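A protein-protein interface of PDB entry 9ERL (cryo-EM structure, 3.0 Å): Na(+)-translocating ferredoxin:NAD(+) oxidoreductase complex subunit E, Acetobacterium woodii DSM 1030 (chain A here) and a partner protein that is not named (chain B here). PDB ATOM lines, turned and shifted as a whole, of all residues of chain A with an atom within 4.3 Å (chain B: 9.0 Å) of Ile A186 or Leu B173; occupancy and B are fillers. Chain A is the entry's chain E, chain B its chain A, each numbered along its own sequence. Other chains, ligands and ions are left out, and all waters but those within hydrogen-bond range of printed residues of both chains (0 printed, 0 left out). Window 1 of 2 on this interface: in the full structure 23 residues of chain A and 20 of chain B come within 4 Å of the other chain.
Among the printed residues, pairs that only touch across the chains: Phe A179 with Leu B173, Phe A179 with Phe B21, Leu A180 with Leu B174, Gly A183 with Leu B173, Gly A183 with Pro B170, Asn A190 with Ala B165, Ile A186 with Pro B170, Phe A179 with Gly B177, Phe A179 with Ala B176, Gly A187 with Pro B170, Leu A180 with Gly B177 and Ile A186 with Leu B173.
Of the printed residues of chain B, Ile A186 touches Pro B170 (3.8 Å) and Leu B173 (3.98 Å). Of the printed residues of chain A, Leu B173 touches Phe A179, Gly A183 and Ile A186. Of the printed residues of chain B, Gly A183 touches Pro B170 (3.7 Å) and Leu B173 (3.7 Å). Gly A187 touches one residue of chain B. No residue of chain B comes within 4 Å of Ile A189. Of the printed residues of chain B, Leu A180 touches Leu B174 (3.6 Å) and Gly B177 (3.9 Å). Of the printed residues of chain A, Ala B176 touches Phe A179. Printed residues of chain B within 4 Å of Asn A190: Ala B165 (3.8 Å). Leu A185 touches none of the printed residues of chain B. Leu A188 touches none of the printed residues of chain B. The nearest printed residue of chain B that does not touch Ile A186 is Phe B169 (4.9 Å). The nearest printed residue of chain A that does not touch Ala B176 is Leu A180 (5.9 Å).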
ATOM      1  N   PHE A  18     -30.447 -21.650 -29.061  1.00  0.00           N
ATOM      2  CA  PHE A  18     -29.465 -20.652 -28.658  1.00  0.00           C
ATOM      3  C   PHE A  18     -29.757 -20.003 -27.312  1.00  0.00           C
ATOM      4  O   PHE A  18     -28.823 -19.509 -26.670  1.00  0.00           O
ATOM      5  CB  PHE A  18     -29.356 -19.555 -29.726  1.00  0.00           C
ATOM      6  CG  PHE A  18     -28.765 -20.028 -31.023  1.00  0.00           C
ATOM      7  CD1 PHE A  18     -27.550 -20.690 -31.045  1.00  0.00           C
ATOM      8  CD2 PHE A  18     -29.421 -19.808 -32.223  1.00  0.00           C
ATOM      9  CE1 PHE A  18     -27.003 -21.128 -32.235  1.00  0.00           C
ATOM     10  CE2 PHE A  18     -28.878 -20.242 -33.417  1.00  0.00           C
ATOM     11  CZ  PHE A  18     -27.668 -20.903 -33.422  1.00  0.00           C
ATOM     12  N   VAL A  21     -31.394 -23.975 -24.933  1.00  0.00           N
ATOM     13  CA  VAL A  21     -30.539 -25.158 -25.018  1.00  0.00           C
ATOM     14  C   VAL A  21     -31.396 -26.375 -24.664  1.00  0.00           C
ATOM     15  O   VAL A  21     -31.404 -26.854 -23.523  1.00  0.00           O
ATOM     16  CB  VAL A  21     -29.272 -24.999 -24.142  1.00  0.00           C
ATOM     17  CG1 VAL A  21     -28.491 -26.316 -23.948  1.00  0.00           C
ATOM     18  CG2 VAL A  21     -28.376 -23.921 -24.724  1.00  0.00           C
ATOM     19  N   PHE A 179     -19.625 -30.060 -30.343  1.00  0.00           N
ATOM     20  CA  PHE A 179     -19.669 -29.339 -29.070  1.00  0.00           C
ATOM     21  C   PHE A 179     -18.984 -27.986 -29.168  1.00  0.00           C
ATOM     22  O   PHE A 179     -19.642 -26.939 -29.074  1.00  0.00           O
ATOM     23  CB  PHE A 179     -18.991 -30.169 -27.980  1.00  0.00           C
ATOM     24  CG  PHE A 179     -19.847 -31.255 -27.402  1.00  0.00           C
ATOM     25  CD1 PHE A 179     -20.969 -30.952 -26.655  1.00  0.00           C
ATOM     26  CD2 PHE A 179     -19.501 -32.583 -27.574  1.00  0.00           C
ATOM     27  CE1 PHE A 179     -21.743 -31.955 -26.111  1.00  0.00           C
ATOM     28  CE2 PHE A 179     -20.269 -33.588 -27.030  1.00  0.00           C
ATOM     29  CZ  PHE A 179     -21.392 -33.275 -26.301  1.00  0.00           C
ATOM     30  N   LEU A 180     -17.672 -28.000 -29.438  1.00  0.00           N
ATOM     31  CA  LEU A 180     -16.887 -26.773 -29.519  1.00  0.00           C
ATOM     32  C   LEU A 180     -17.538 -25.767 -30.453  1.00  0.00           C
ATOM     33  O   LEU A 180     -17.795 -24.622 -30.050  1.00  0.00           O
ATOM     34  CB  LEU A 180     -15.466 -27.087 -29.987  1.00  0.00           C
ATOM     35  CG  LEU A 180     -14.770 -28.322 -29.414  1.00  0.00           C
ATOM     36  CD1 LEU A 180     -13.518 -28.647 -30.208  1.00  0.00           C
ATOM     37  CD2 LEU A 180     -14.425 -28.112 -27.953  1.00  0.00           C
ATOM     38  N   LEU A 182     -20.656 -25.428 -31.487  1.00  0.00           N
ATOM     39  CA  LEU A 182     -21.873 -24.863 -30.922  1.00  0.00           C
ATOM     40  C   LEU A 182     -21.538 -23.855 -29.838  1.00  0.00           C
ATOM     41  O   LEU A 182     -22.047 -22.726 -29.862  1.00  0.00           O
ATOM     42  CB  LEU A 182     -22.771 -25.971 -30.376  1.00  0.00           C
ATOM     43  CG  LEU A 182     -24.212 -25.572 -30.053  1.00  0.00           C
ATOM     44  CD1 LEU A 182     -24.852 -24.859 -31.230  1.00  0.00           C
ATOM     45  CD2 LEU A 182     -25.027 -26.790 -29.661  1.00  0.00           C
ATOM     46  N   GLY A 183     -20.595 -24.212 -28.956  1.00  0.00           N
ATOM     47  CA  GLY A 183     -20.232 -23.310 -27.881  1.00  0.00           C
ATOM     48  C   GLY A 183     -19.778 -21.969 -28.410  1.00  0.00           C
ATOM     49  O   GLY A 183     -20.304 -20.925 -28.006  1.00  0.00           O
ATOM     50  N   LEU A 184     -18.901 -21.992 -29.421  1.00  0.00           N
ATOM     51  CA  LEU A 184     -18.391 -20.744 -29.973  1.00  0.00           C
ATOM     52  C   LEU A 184     -19.531 -19.895 -30.505  1.00  0.00           C
ATOM     53  O   LEU A 184     -19.629 -18.705 -30.170  1.00  0.00           O
ATOM     54  CB  LEU A 184     -17.362 -21.029 -31.065  1.00  0.00           C
ATOM     55  CG  LEU A 184     -16.024 -21.599 -30.587  1.00  0.00           C
ATOM     56  CD1 LEU A 184     -15.118 -21.910 -31.765  1.00  0.00           C
ATOM     57  CD2 LEU A 184     -15.342 -20.643 -29.624  1.00  0.00           C
ATOM     58  N   LEU A 185     -20.466 -20.524 -31.231  1.00  0.00           N
ATOM     59  CA  LEU A 185     -21.593 -19.779 -31.776  1.00  0.00           C
ATOM     60  C   LEU A 185     -22.375 -19.106 -30.664  1.00  0.00           C
ATOM     61  O   LEU A 185     -22.608 -17.888 -30.714  1.00  0.00           O
ATOM     62  CB  LEU A 185     -22.498 -20.702 -32.591  1.00  0.00           C
ATOM     63  CG  LEU A 185     -22.056 -20.982 -34.028  1.00  0.00           C
ATOM     64  CD1 LEU A 185     -23.042 -21.904 -34.723  1.00  0.00           C
ATOM     65  CD2 LEU A 185     -21.901 -19.682 -34.798  1.00  0.00           C
ATOM     66  N   ILE A 186     -22.680 -19.856 -29.598  1.00  0.00           N
ATOM     67  CA  ILE A 186     -23.443 -19.283 -28.498  1.00  0.00           C
ATOM     68  C   ILE A 186     -22.688 -18.105 -27.910  1.00  0.00           C
ATOM     69  O   ILE A 186     -23.257 -17.018 -27.730  1.00  0.00           O
ATOM     70  CB  ILE A 186     -23.760 -20.352 -27.437  1.00  0.00           C
ATOM     71  CG1 ILE A 186     -24.745 -21.380 -27.993  1.00  0.00           C
ATOM     72  CG2 ILE A 186     -24.328 -19.709 -26.186  1.00  0.00           C
ATOM     73  CD1 ILE A 186     -25.152 -22.437 -26.993  1.00  0.00           C
ATOM     74  N   GLY A 187     -21.373 -18.270 -27.718  1.00  0.00           N
ATOM     75  CA  GLY A 187     -20.576 -17.189 -27.170  1.00  0.00           C
ATOM     76  C   GLY A 187     -20.689 -15.935 -28.005  1.00  0.00           C
ATOM     77  O   GLY A 187     -20.973 -14.854 -27.476  1.00  0.00           O
ATOM     78  N   LEU A 188     -20.591 -16.088 -29.333  1.00  0.00           N
ATOM     79  CA  LEU A 188     -20.687 -14.933 -30.215  1.00  0.00           C
ATOM     80  C   LEU A 188     -22.008 -14.217 -30.010  1.00  0.00           C
ATOM     81  O   LEU A 188     -22.031 -13.001 -29.771  1.00  0.00           O
ATOM     82  CB  LEU A 188     -20.528 -15.369 -31.671  1.00  0.00           C
ATOM     83  CG  LEU A 188     -20.531 -14.266 -32.730  1.00  0.00           C
ATOM     84  CD1 LEU A 188     -19.301 -13.385 -32.594  1.00  0.00           C
ATOM     85  CD2 LEU A 188     -20.611 -14.866 -34.123  1.00  0.00           C
ATOM     86  N   ILE A 189     -23.106 -14.981 -29.975  1.00  0.00           N
ATOM     87  CA  ILE A 189     -24.421 -14.378 -29.797  1.00  0.00           C
ATOM     88  C   ILE A 189     -24.467 -13.627 -28.479  1.00  0.00           C
ATOM     89  O   ILE A 189     -24.863 -12.452 -28.433  1.00  0.00           O
ATOM     90  CB  ILE A 189     -25.519 -15.453 -29.887  1.00  0.00           C
ATOM     91  CG1 ILE A 189     -25.687 -15.914 -31.335  1.00  0.00           C
ATOM     92  CG2 ILE A 189     -26.833 -14.928 -29.342  1.00  0.00           C
ATOM     93  CD1 ILE A 189     -26.465 -17.197 -31.481  1.00  0.00           C
ATOM     94  N   ASN A 190     -23.952 -14.253 -27.411  1.00  0.00           N
ATOM     95  CA  ASN A 190     -23.975 -13.614 -26.101  1.00  0.00           C
ATOM     96  C   ASN A 190     -23.218 -12.300 -26.138  1.00  0.00           C
ATOM     97  O   ASN A 190     -23.698 -11.286 -25.614  1.00  0.00           O
ATOM     98  CB  ASN A 190     -23.388 -14.547 -25.044  1.00  0.00           C
ATOM     99  CG  ASN A 190     -24.396 -15.556 -24.533  1.00  0.00           C
ATOM    100  OD1 ASN A 190     -25.491 -15.684 -25.075  1.00  0.00           O
ATOM    101  ND2 ASN A 190     -24.028 -16.275 -23.480  1.00  0.00           N
ATOM    102  N   LEU B  18     -20.702 -39.580 -23.983  1.00  0.00           N
ATOM    103  CA  LEU B  18     -19.597 -38.990 -24.728  1.00  0.00           C
ATOM    104  C   LEU B  18     -19.427 -39.574 -26.124  1.00  0.00           C
ATOM    105  O   LEU B  18     -18.628 -39.040 -26.902  1.00  0.00           O
ATOM    106  CB  LEU B  18     -18.299 -39.149 -23.935  1.00  0.00           C
ATOM    107  CG  LEU B  18     -18.193 -38.279 -22.679  1.00  0.00           C
ATOM    108  CD1 LEU B  18     -16.832 -38.428 -22.031  1.00  0.00           C
ATOM    109  CD2 LEU B  18     -18.473 -36.821 -23.003  1.00  0.00           C
ATOM    110  N   PHE B  21     -24.341 -39.723 -27.927  1.00  0.00           N
ATOM    111  CA  PHE B  21     -25.137 -38.490 -27.943  1.00  0.00           C
ATOM    112  C   PHE B  21     -26.564 -38.724 -27.441  1.00  0.00           C
ATOM    113  O   PHE B  21     -27.542 -38.453 -28.138  1.00  0.00           O
ATOM    114  CB  PHE B  21     -25.168 -37.876 -29.349  1.00  0.00           C
ATOM    115  CG  PHE B  21     -24.007 -36.983 -29.659  1.00  0.00           C
ATOM    116  CD1 PHE B  21     -23.522 -36.095 -28.720  1.00  0.00           C
ATOM    117  CD2 PHE B  21     -23.406 -37.029 -30.905  1.00  0.00           C
ATOM    118  CE1 PHE B  21     -22.459 -35.273 -29.014  1.00  0.00           C
ATOM    119  CE2 PHE B  21     -22.341 -36.209 -31.204  1.00  0.00           C
ATOM    120  CZ  PHE B  21     -21.866 -35.330 -30.257  1.00  0.00           C
ATOM    121  N   ILE B  24     -27.636 -35.733 -22.897  1.00  0.00           N
ATOM    122  CA  ILE B  24     -26.927 -34.461 -22.993  1.00  0.00           C
ATOM    123  C   ILE B  24     -27.590 -33.366 -22.162  1.00  0.00           C
ATOM    124  O   ILE B  24     -26.900 -32.602 -21.487  1.00  0.00           O
ATOM    125  CB  ILE B  24     -26.791 -34.035 -24.469  1.00  0.00           C
ATOM    126  CG1 ILE B  24     -25.843 -34.977 -25.203  1.00  0.00           C
ATOM    127  CG2 ILE B  24     -26.251 -32.622 -24.579  1.00  0.00           C
ATOM    128  CD1 ILE B  24     -26.264 -35.262 -26.611  1.00  0.00           C
ATOM    129  N   PHE B  27     -27.002 -33.710 -18.583  1.00  0.00           N
ATOM    130  CA  PHE B  27     -25.556 -33.586 -18.433  1.00  0.00           C
ATOM    131  C   PHE B  27     -25.151 -32.132 -18.245  1.00  0.00           C
ATOM    132  O   PHE B  27     -24.281 -31.822 -17.423  1.00  0.00           O
ATOM    133  CB  PHE B  27     -24.863 -34.186 -19.658  1.00  0.00           C
ATOM    134  CG  PHE B  27     -23.400 -34.453 -19.475  1.00  0.00           C
ATOM    135  CD1 PHE B  27     -22.953 -35.301 -18.481  1.00  0.00           C
ATOM    136  CD2 PHE B  27     -22.472 -33.872 -20.322  1.00  0.00           C
ATOM    137  CE1 PHE B  27     -21.605 -35.551 -18.327  1.00  0.00           C
ATOM    138  CE2 PHE B  27     -21.126 -34.119 -20.171  1.00  0.00           C
ATOM    139  CZ  PHE B  27     -20.692 -34.959 -19.172  1.00  0.00           C
ATOM    140  N   LEU B  28     -25.768 -31.224 -19.000  1.00  0.00           N
ATOM    141  CA  LEU B  28     -25.486 -29.802 -18.860  1.00  0.00           C
ATOM    142  C   LEU B  28     -26.350 -29.133 -17.802  1.00  0.00           C
ATOM    143  O   LEU B  28     -26.024 -28.024 -17.368  1.00  0.00           O
ATOM    144  CB  LEU B  28     -25.686 -29.093 -20.201  1.00  0.00           C
ATOM    145  CG  LEU B  28     -24.861 -29.600 -21.384  1.00  0.00           C
ATOM    146  CD1 LEU B  28     -25.268 -28.886 -22.659  1.00  0.00           C
ATOM    147  CD2 LEU B  28     -23.380 -29.423 -21.119  1.00  0.00           C
ATOM    148  N   PHE B 150     -17.723 -34.564 -14.914  1.00  0.00           N
ATOM    149  CA  PHE B 150     -18.070 -33.223 -15.381  1.00  0.00           C
ATOM    150  C   PHE B 150     -18.294 -32.263 -14.219  1.00  0.00           C
ATOM    151  O   PHE B 150     -17.842 -31.110 -14.260  1.00  0.00           O
ATOM    152  CB  PHE B 150     -19.315 -33.289 -16.265  1.00  0.00           C
ATOM    153  CG  PHE B 150     -19.484 -32.101 -17.166  1.00  0.00           C
ATOM    154  CD1 PHE B 150     -18.384 -31.411 -17.642  1.00  0.00           C
ATOM    155  CD2 PHE B 150     -20.747 -31.673 -17.535  1.00  0.00           C
ATOM    156  CE1 PHE B 150     -18.541 -30.320 -18.470  1.00  0.00           C
ATOM    157  CE2 PHE B 150     -20.909 -30.583 -18.363  1.00  0.00           C
ATOM    158  CZ  PHE B 150     -19.805 -29.906 -18.831  1.00  0.00           C
ATOM    159  N   ARG B 154     -16.150 -28.826 -13.423  1.00  0.00           N
ATOM    160  CA  ARG B 154     -16.789 -27.517 -13.280  1.00  0.00           C
ATOM    161  C   ARG B 154     -16.463 -26.875 -11.933  1.00  0.00           C
ATOM    162  O   ARG B 154     -16.214 -25.662 -11.855  1.00  0.00           O
ATOM    163  CB  ARG B 154     -18.298 -27.652 -13.467  1.00  0.00           C
ATOM    164  CG  ARG B 154     -18.716 -27.896 -14.907  1.00  0.00           C
ATOM    165  CD  ARG B 154     -20.227 -27.913 -15.048  1.00  0.00           C
ATOM    166  NE  ARG B 154     -20.760 -26.602 -15.396  1.00  0.00           N
ATOM    167  CZ  ARG B 154     -22.008 -26.381 -15.785  1.00  0.00           C
ATOM    168  NH1 ARG B 154     -22.884 -27.364 -15.888  1.00  0.00           N
ATOM    169  NH2 ARG B 154     -22.386 -25.139 -16.074  1.00  0.00           N
ATOM    170  N   LEU B 157     -13.128 -25.439 -12.291  1.00  0.00           N
ATOM    171  CA  LEU B 157     -13.146 -24.243 -13.129  1.00  0.00           C
ATOM    172  C   LEU B 157     -13.823 -23.057 -12.461  1.00  0.00           C
ATOM    173  O   LEU B 157     -13.770 -21.951 -13.006  1.00  0.00           O
ATOM    174  CB  LEU B 157     -13.848 -24.528 -14.457  1.00  0.00           C
ATOM    175  CG  LEU B 157     -13.042 -25.180 -15.578  1.00  0.00           C
ATOM    176  CD1 LEU B 157     -13.849 -25.160 -16.862  1.00  0.00           C
ATOM    177  CD2 LEU B 157     -11.706 -24.481 -15.765  1.00  0.00           C
ATOM    178  N   ALA B 165     -17.897 -13.430 -21.493  1.00  0.00           N
ATOM    179  CA  ALA B 165     -18.890 -13.753 -22.507  1.00  0.00           C
ATOM    180  C   ALA B 165     -19.165 -15.237 -22.656  1.00  0.00           C
ATOM    181  O   ALA B 165     -20.258 -15.600 -23.099  1.00  0.00           O
ATOM    182  CB  ALA B 165     -18.461 -13.194 -23.871  1.00  0.00           C
ATOM    183  N   LEU B 166     -18.212 -16.099 -22.308  1.00  0.00           N
ATOM    184  CA  LEU B 166     -18.468 -17.530 -22.384  1.00  0.00           C
ATOM    185  C   LEU B 166     -19.303 -17.988 -21.194  1.00  0.00           C
ATOM    186  O   LEU B 166     -20.468 -18.364 -21.354  1.00  0.00           O
ATOM    187  CB  LEU B 166     -17.143 -18.291 -22.466  1.00  0.00           C
ATOM    188  CG  LEU B 166     -16.241 -17.866 -23.629  1.00  0.00           C
ATOM    189  CD1 LEU B 166     -14.981 -18.706 -23.675  1.00  0.00           C
ATOM    190  CD2 LEU B 166     -16.982 -17.947 -24.952  1.00  0.00           C
ATOM    191  N   GLU B 167     -18.742 -17.897 -19.988  1.00  0.00           N
ATOM    192  CA  GLU B 167     -19.426 -18.217 -18.722  1.00  0.00           C
ATOM    193  C   GLU B 167     -19.965 -19.647 -18.800  1.00  0.00           C
ATOM    194  O   GLU B 167     -19.200 -20.560 -19.134  1.00  0.00           O
ATOM    195  CB  GLU B 167     -20.456 -17.139 -18.415  1.00  0.00           C
ATOM    196  CG  GLU B 167     -19.861 -15.748 -18.224  1.00  0.00           C
ATOM    197  CD  GLU B 167     -19.398 -15.484 -16.798  1.00  0.00           C
ATOM    198  OE1 GLU B 167     -18.979 -16.436 -16.108  1.00  0.00           O
ATOM    199  OE2 GLU B 167     -19.460 -14.315 -16.365  1.00  0.00           O
ATOM    200  N   GLY B 168     -21.245 -19.886 -18.514  1.00  0.00           N
ATOM    201  CA  GLY B 168     -21.735 -21.235 -18.296  1.00  0.00           C
ATOM    202  C   GLY B 168     -21.768 -22.187 -19.477  1.00  0.00           C
ATOM    203  O   GLY B 168     -20.962 -23.122 -19.540  1.00  0.00           O
ATOM    204  N   PHE B 169     -22.680 -21.959 -20.425  1.00  0.00           N
ATOM    205  CA  PHE B 169     -22.963 -22.954 -21.459  1.00  0.00           C
ATOM    206  C   PHE B 169     -21.855 -23.085 -22.508  1.00  0.00           C
ATOM    207  O   PHE B 169     -21.527 -24.220 -22.883  1.00  0.00           O
ATOM    208  CB  PHE B 169     -24.310 -22.661 -22.133  1.00  0.00           C
ATOM    209  CG  PHE B 169     -25.493 -23.210 -21.390  1.00  0.00           C
ATOM    210  CD1 PHE B 169     -25.561 -24.553 -21.065  1.00  0.00           C
ATOM    211  CD2 PHE B 169     -26.542 -22.384 -21.022  1.00  0.00           C
ATOM    212  CE1 PHE B 169     -26.649 -25.062 -20.381  1.00  0.00           C
ATOM    213  CE2 PHE B 169     -27.632 -22.887 -20.340  1.00  0.00           C
ATOM    214  CZ  PHE B 169     -27.686 -24.228 -20.020  1.00  0.00           C
ATOM    215  N   PRO B 170     -21.270 -21.994 -23.038  1.00  0.00           N
ATOM    216  CA  PRO B 170     -20.116 -22.182 -23.939  1.00  0.00           C
ATOM    217  C   PRO B 170     -18.945 -22.923 -23.314  1.00  0.00           C
ATOM    218  O   PRO B 170     -18.357 -23.796 -23.969  1.00  0.00           O
ATOM    219  CB  PRO B 170     -19.741 -20.744 -24.316  1.00  0.00           C
ATOM    220  CG  PRO B 170     -21.015 -20.021 -24.267  1.00  0.00           C
ATOM    221  CD  PRO B 170     -21.758 -20.601 -23.105  1.00  0.00           C
ATOM    222  N   ILE B 171     -18.597 -22.629 -22.058  1.00  0.00           N
ATOM    223  CA  ILE B 171     -17.462 -23.328 -21.464  1.00  0.00           C
ATOM    224  C   ILE B 171     -17.842 -24.763 -21.116  1.00  0.00           C
ATOM    225  O   ILE B 171     -16.990 -25.661 -21.165  1.00  0.00           O
ATOM    226  CB  ILE B 171     -16.902 -22.549 -20.257  1.00  0.00           C
ATOM    227  CG1 ILE B 171     -15.374 -22.550 -20.299  1.00  0.00           C
ATOM    228  CG2 ILE B 171     -17.354 -23.146 -18.933  1.00  0.00           C
ATOM    229  CD1 ILE B 171     -14.790 -21.640 -21.349  1.00  0.00           C
ATOM    230  N   ALA B 172     -19.120 -25.021 -20.810  1.00  0.00           N
ATOM    231  CA  ALA B 172     -19.559 -26.398 -20.613  1.00  0.00           C
ATOM    232  C   ALA B 172     -19.442 -27.200 -21.902  1.00  0.00           C
ATOM    233  O   ALA B 172     -18.997 -28.354 -21.885  1.00  0.00           O
ATOM    234  CB  ALA B 172     -20.994 -26.423 -20.091  1.00  0.00           C
ATOM    235  N   LEU B 173     -19.817 -26.596 -23.031  1.00  0.00           N
ATOM    236  CA  LEU B 173     -19.715 -27.293 -24.310  1.00  0.00           C
ATOM    237  C   LEU B 173     -18.259 -27.525 -24.710  1.00  0.00           C
ATOM    238  O   LEU B 173     -17.917 -28.593 -25.231  1.00  0.00           O
ATOM    239  CB  LEU B 173     -20.468 -26.516 -25.388  1.00  0.00           C
ATOM    240  CG  LEU B 173     -21.992 -26.526 -25.224  1.00  0.00           C
ATOM    241  CD1 LEU B 173     -22.622 -25.275 -25.813  1.00  0.00           C
ATOM    242  CD2 LEU B 173     -22.603 -27.772 -25.841  1.00  0.00           C
ATOM    243  N   LEU B 174     -17.382 -26.545 -24.463  1.00  0.00           N
ATOM    244  CA  LEU B 174     -15.963 -26.741 -24.763  1.00  0.00           C
ATOM    245  C   LEU B 174     -15.350 -27.836 -23.891  1.00  0.00           C
ATOM    246  O   LEU B 174     -14.560 -28.662 -24.377  1.00  0.00           O
ATOM    247  CB  LEU B 174     -15.200 -25.428 -24.594  1.00  0.00           C
ATOM    248  CG  LEU B 174     -15.537 -24.291 -25.564  1.00  0.00           C
ATOM    249  CD1 LEU B 174     -15.172 -22.946 -24.963  1.00  0.00           C
ATOM    250  CD2 LEU B 174     -14.838 -24.484 -26.897  1.00  0.00           C
ATOM    251  N   THR B 175     -15.704 -27.862 -22.601  1.00  0.00           N
ATOM    252  CA  THR B 175     -15.225 -28.919 -21.716  1.00  0.00           C
ATOM    253  C   THR B 175     -15.721 -30.287 -22.167  1.00  0.00           C
ATOM    254  O   THR B 175     -14.968 -31.271 -22.144  1.00  0.00           O
ATOM    255  CB  THR B 175     -15.676 -28.633 -20.284  1.00  0.00           C
ATOM    256  OG1 THR B 175     -15.272 -27.312 -19.908  1.00  0.00           O
ATOM    257  CG2 THR B 175     -15.070 -29.634 -19.325  1.00  0.00           C
ATOM    258  N   ALA B 176     -16.988 -30.367 -22.584  1.00  0.00           N
ATOM    259  CA  ALA B 176     -17.527 -31.626 -23.087  1.00  0.00           C
ATOM    260  C   ALA B 176     -16.803 -32.073 -24.350  1.00  0.00           C
ATOM    261  O   ALA B 176     -16.561 -33.269 -24.540  1.00  0.00           O
ATOM    262  CB  ALA B 176     -19.026 -31.488 -23.342  1.00  0.00           C
ATOM    263  N   GLY B 177     -16.442 -31.129 -25.222  1.00  0.00           N
ATOM    264  CA  GLY B 177     -15.687 -31.487 -26.415  1.00  0.00           C
ATOM    265  C   GLY B 177     -14.304 -32.031 -26.103  1.00  0.00           C
ATOM    266  O   GLY B 177     -13.849 -32.999 -26.723  1.00  0.00           O
ATOM    267  N   LEU B 178     -13.614 -31.416 -25.139  1.00  0.00           N
ATOM    268  CA  LEU B 178     -12.297 -31.924 -24.746  1.00  0.00           C
ATOM    269  C   LEU B 178     -12.394 -33.314 -24.116  1.00  0.00           C
ATOM    270  O   LEU B 178     -11.570 -34.199 -24.404  1.00  0.00           O
ATOM    271  CB  LEU B 178     -11.618 -30.938 -23.797  1.00  0.00           C
ATOM    272  CG  LEU B 178     -11.329 -29.557 -24.388  1.00  0.00           C
ATOM    273  CD1 LEU B 178     -10.739 -28.629 -23.342  1.00  0.00           C
ATOM    274  CD2 LEU B 178     -10.407 -29.663 -25.590  1.00  0.00           C
ATOM    275  N   MET B 179     -13.401 -33.531 -23.263  1.00  0.00           N
ATOM    276  CA  MET B 179     -13.619 -34.861 -22.696  1.00  0.00           C
ATOM    277  C   MET B 179     -13.949 -35.878 -23.783  1.00  0.00           C
ATOM    278  O   MET B 179     -13.522 -37.039 -23.713  1.00  0.00           O
ATOM    279  CB  MET B 179     -14.737 -34.813 -21.657  1.00  0.00           C
ATOM    280  CG  MET B 179     -14.390 -34.057 -20.389  1.00  0.00           C
ATOM    281  SD  MET B 179     -15.803 -33.904 -19.281  1.00  0.00           S
ATOM    282  CE  MET B 179     -16.042 -35.609 -18.796  1.00  0.00           C
ATOM    283  N   ALA B 180     -14.713 -35.461 -24.796  1.00  0.00           N
ATOM    284  CA  ALA B 180     -15.040 -36.346 -25.906  1.00  0.00           C
ATOM    285  C   ALA B 180     -13.806 -36.725 -26.711  1.00  0.00           C
ATOM    286  O   ALA B 180     -13.711 -37.858 -27.181  1.00  0.00           O
ATOM    287  CB  ALA B 180     -16.086 -35.694 -26.808  1.00  0.00           C
ATOM    288  N   ILE B 181     -12.861 -35.797 -26.891  1.00  0.00           N
ATOM    289  CA  ILE B 181     -11.596 -36.150 -27.540  1.00  0.00           C
ATOM    290  C   ILE B 181     -10.836 -37.181 -26.711  1.00  0.00           C
ATOM    291  O   ILE B 181     -10.349 -38.204 -27.233  1.00  0.00           O
ATOM    292  CB  ILE B 181     -10.745 -34.888 -27.777  1.00  0.00           C
ATOM    293  CG1 ILE B 181     -11.382 -33.992 -28.840  1.00  0.00           C
ATOM    294  CG2 ILE B 181      -9.327 -35.263 -28.175  1.00  0.00           C
ATOM    295  CD1 ILE B 181     -10.516 -32.813 -29.241  1.00  0.00           C
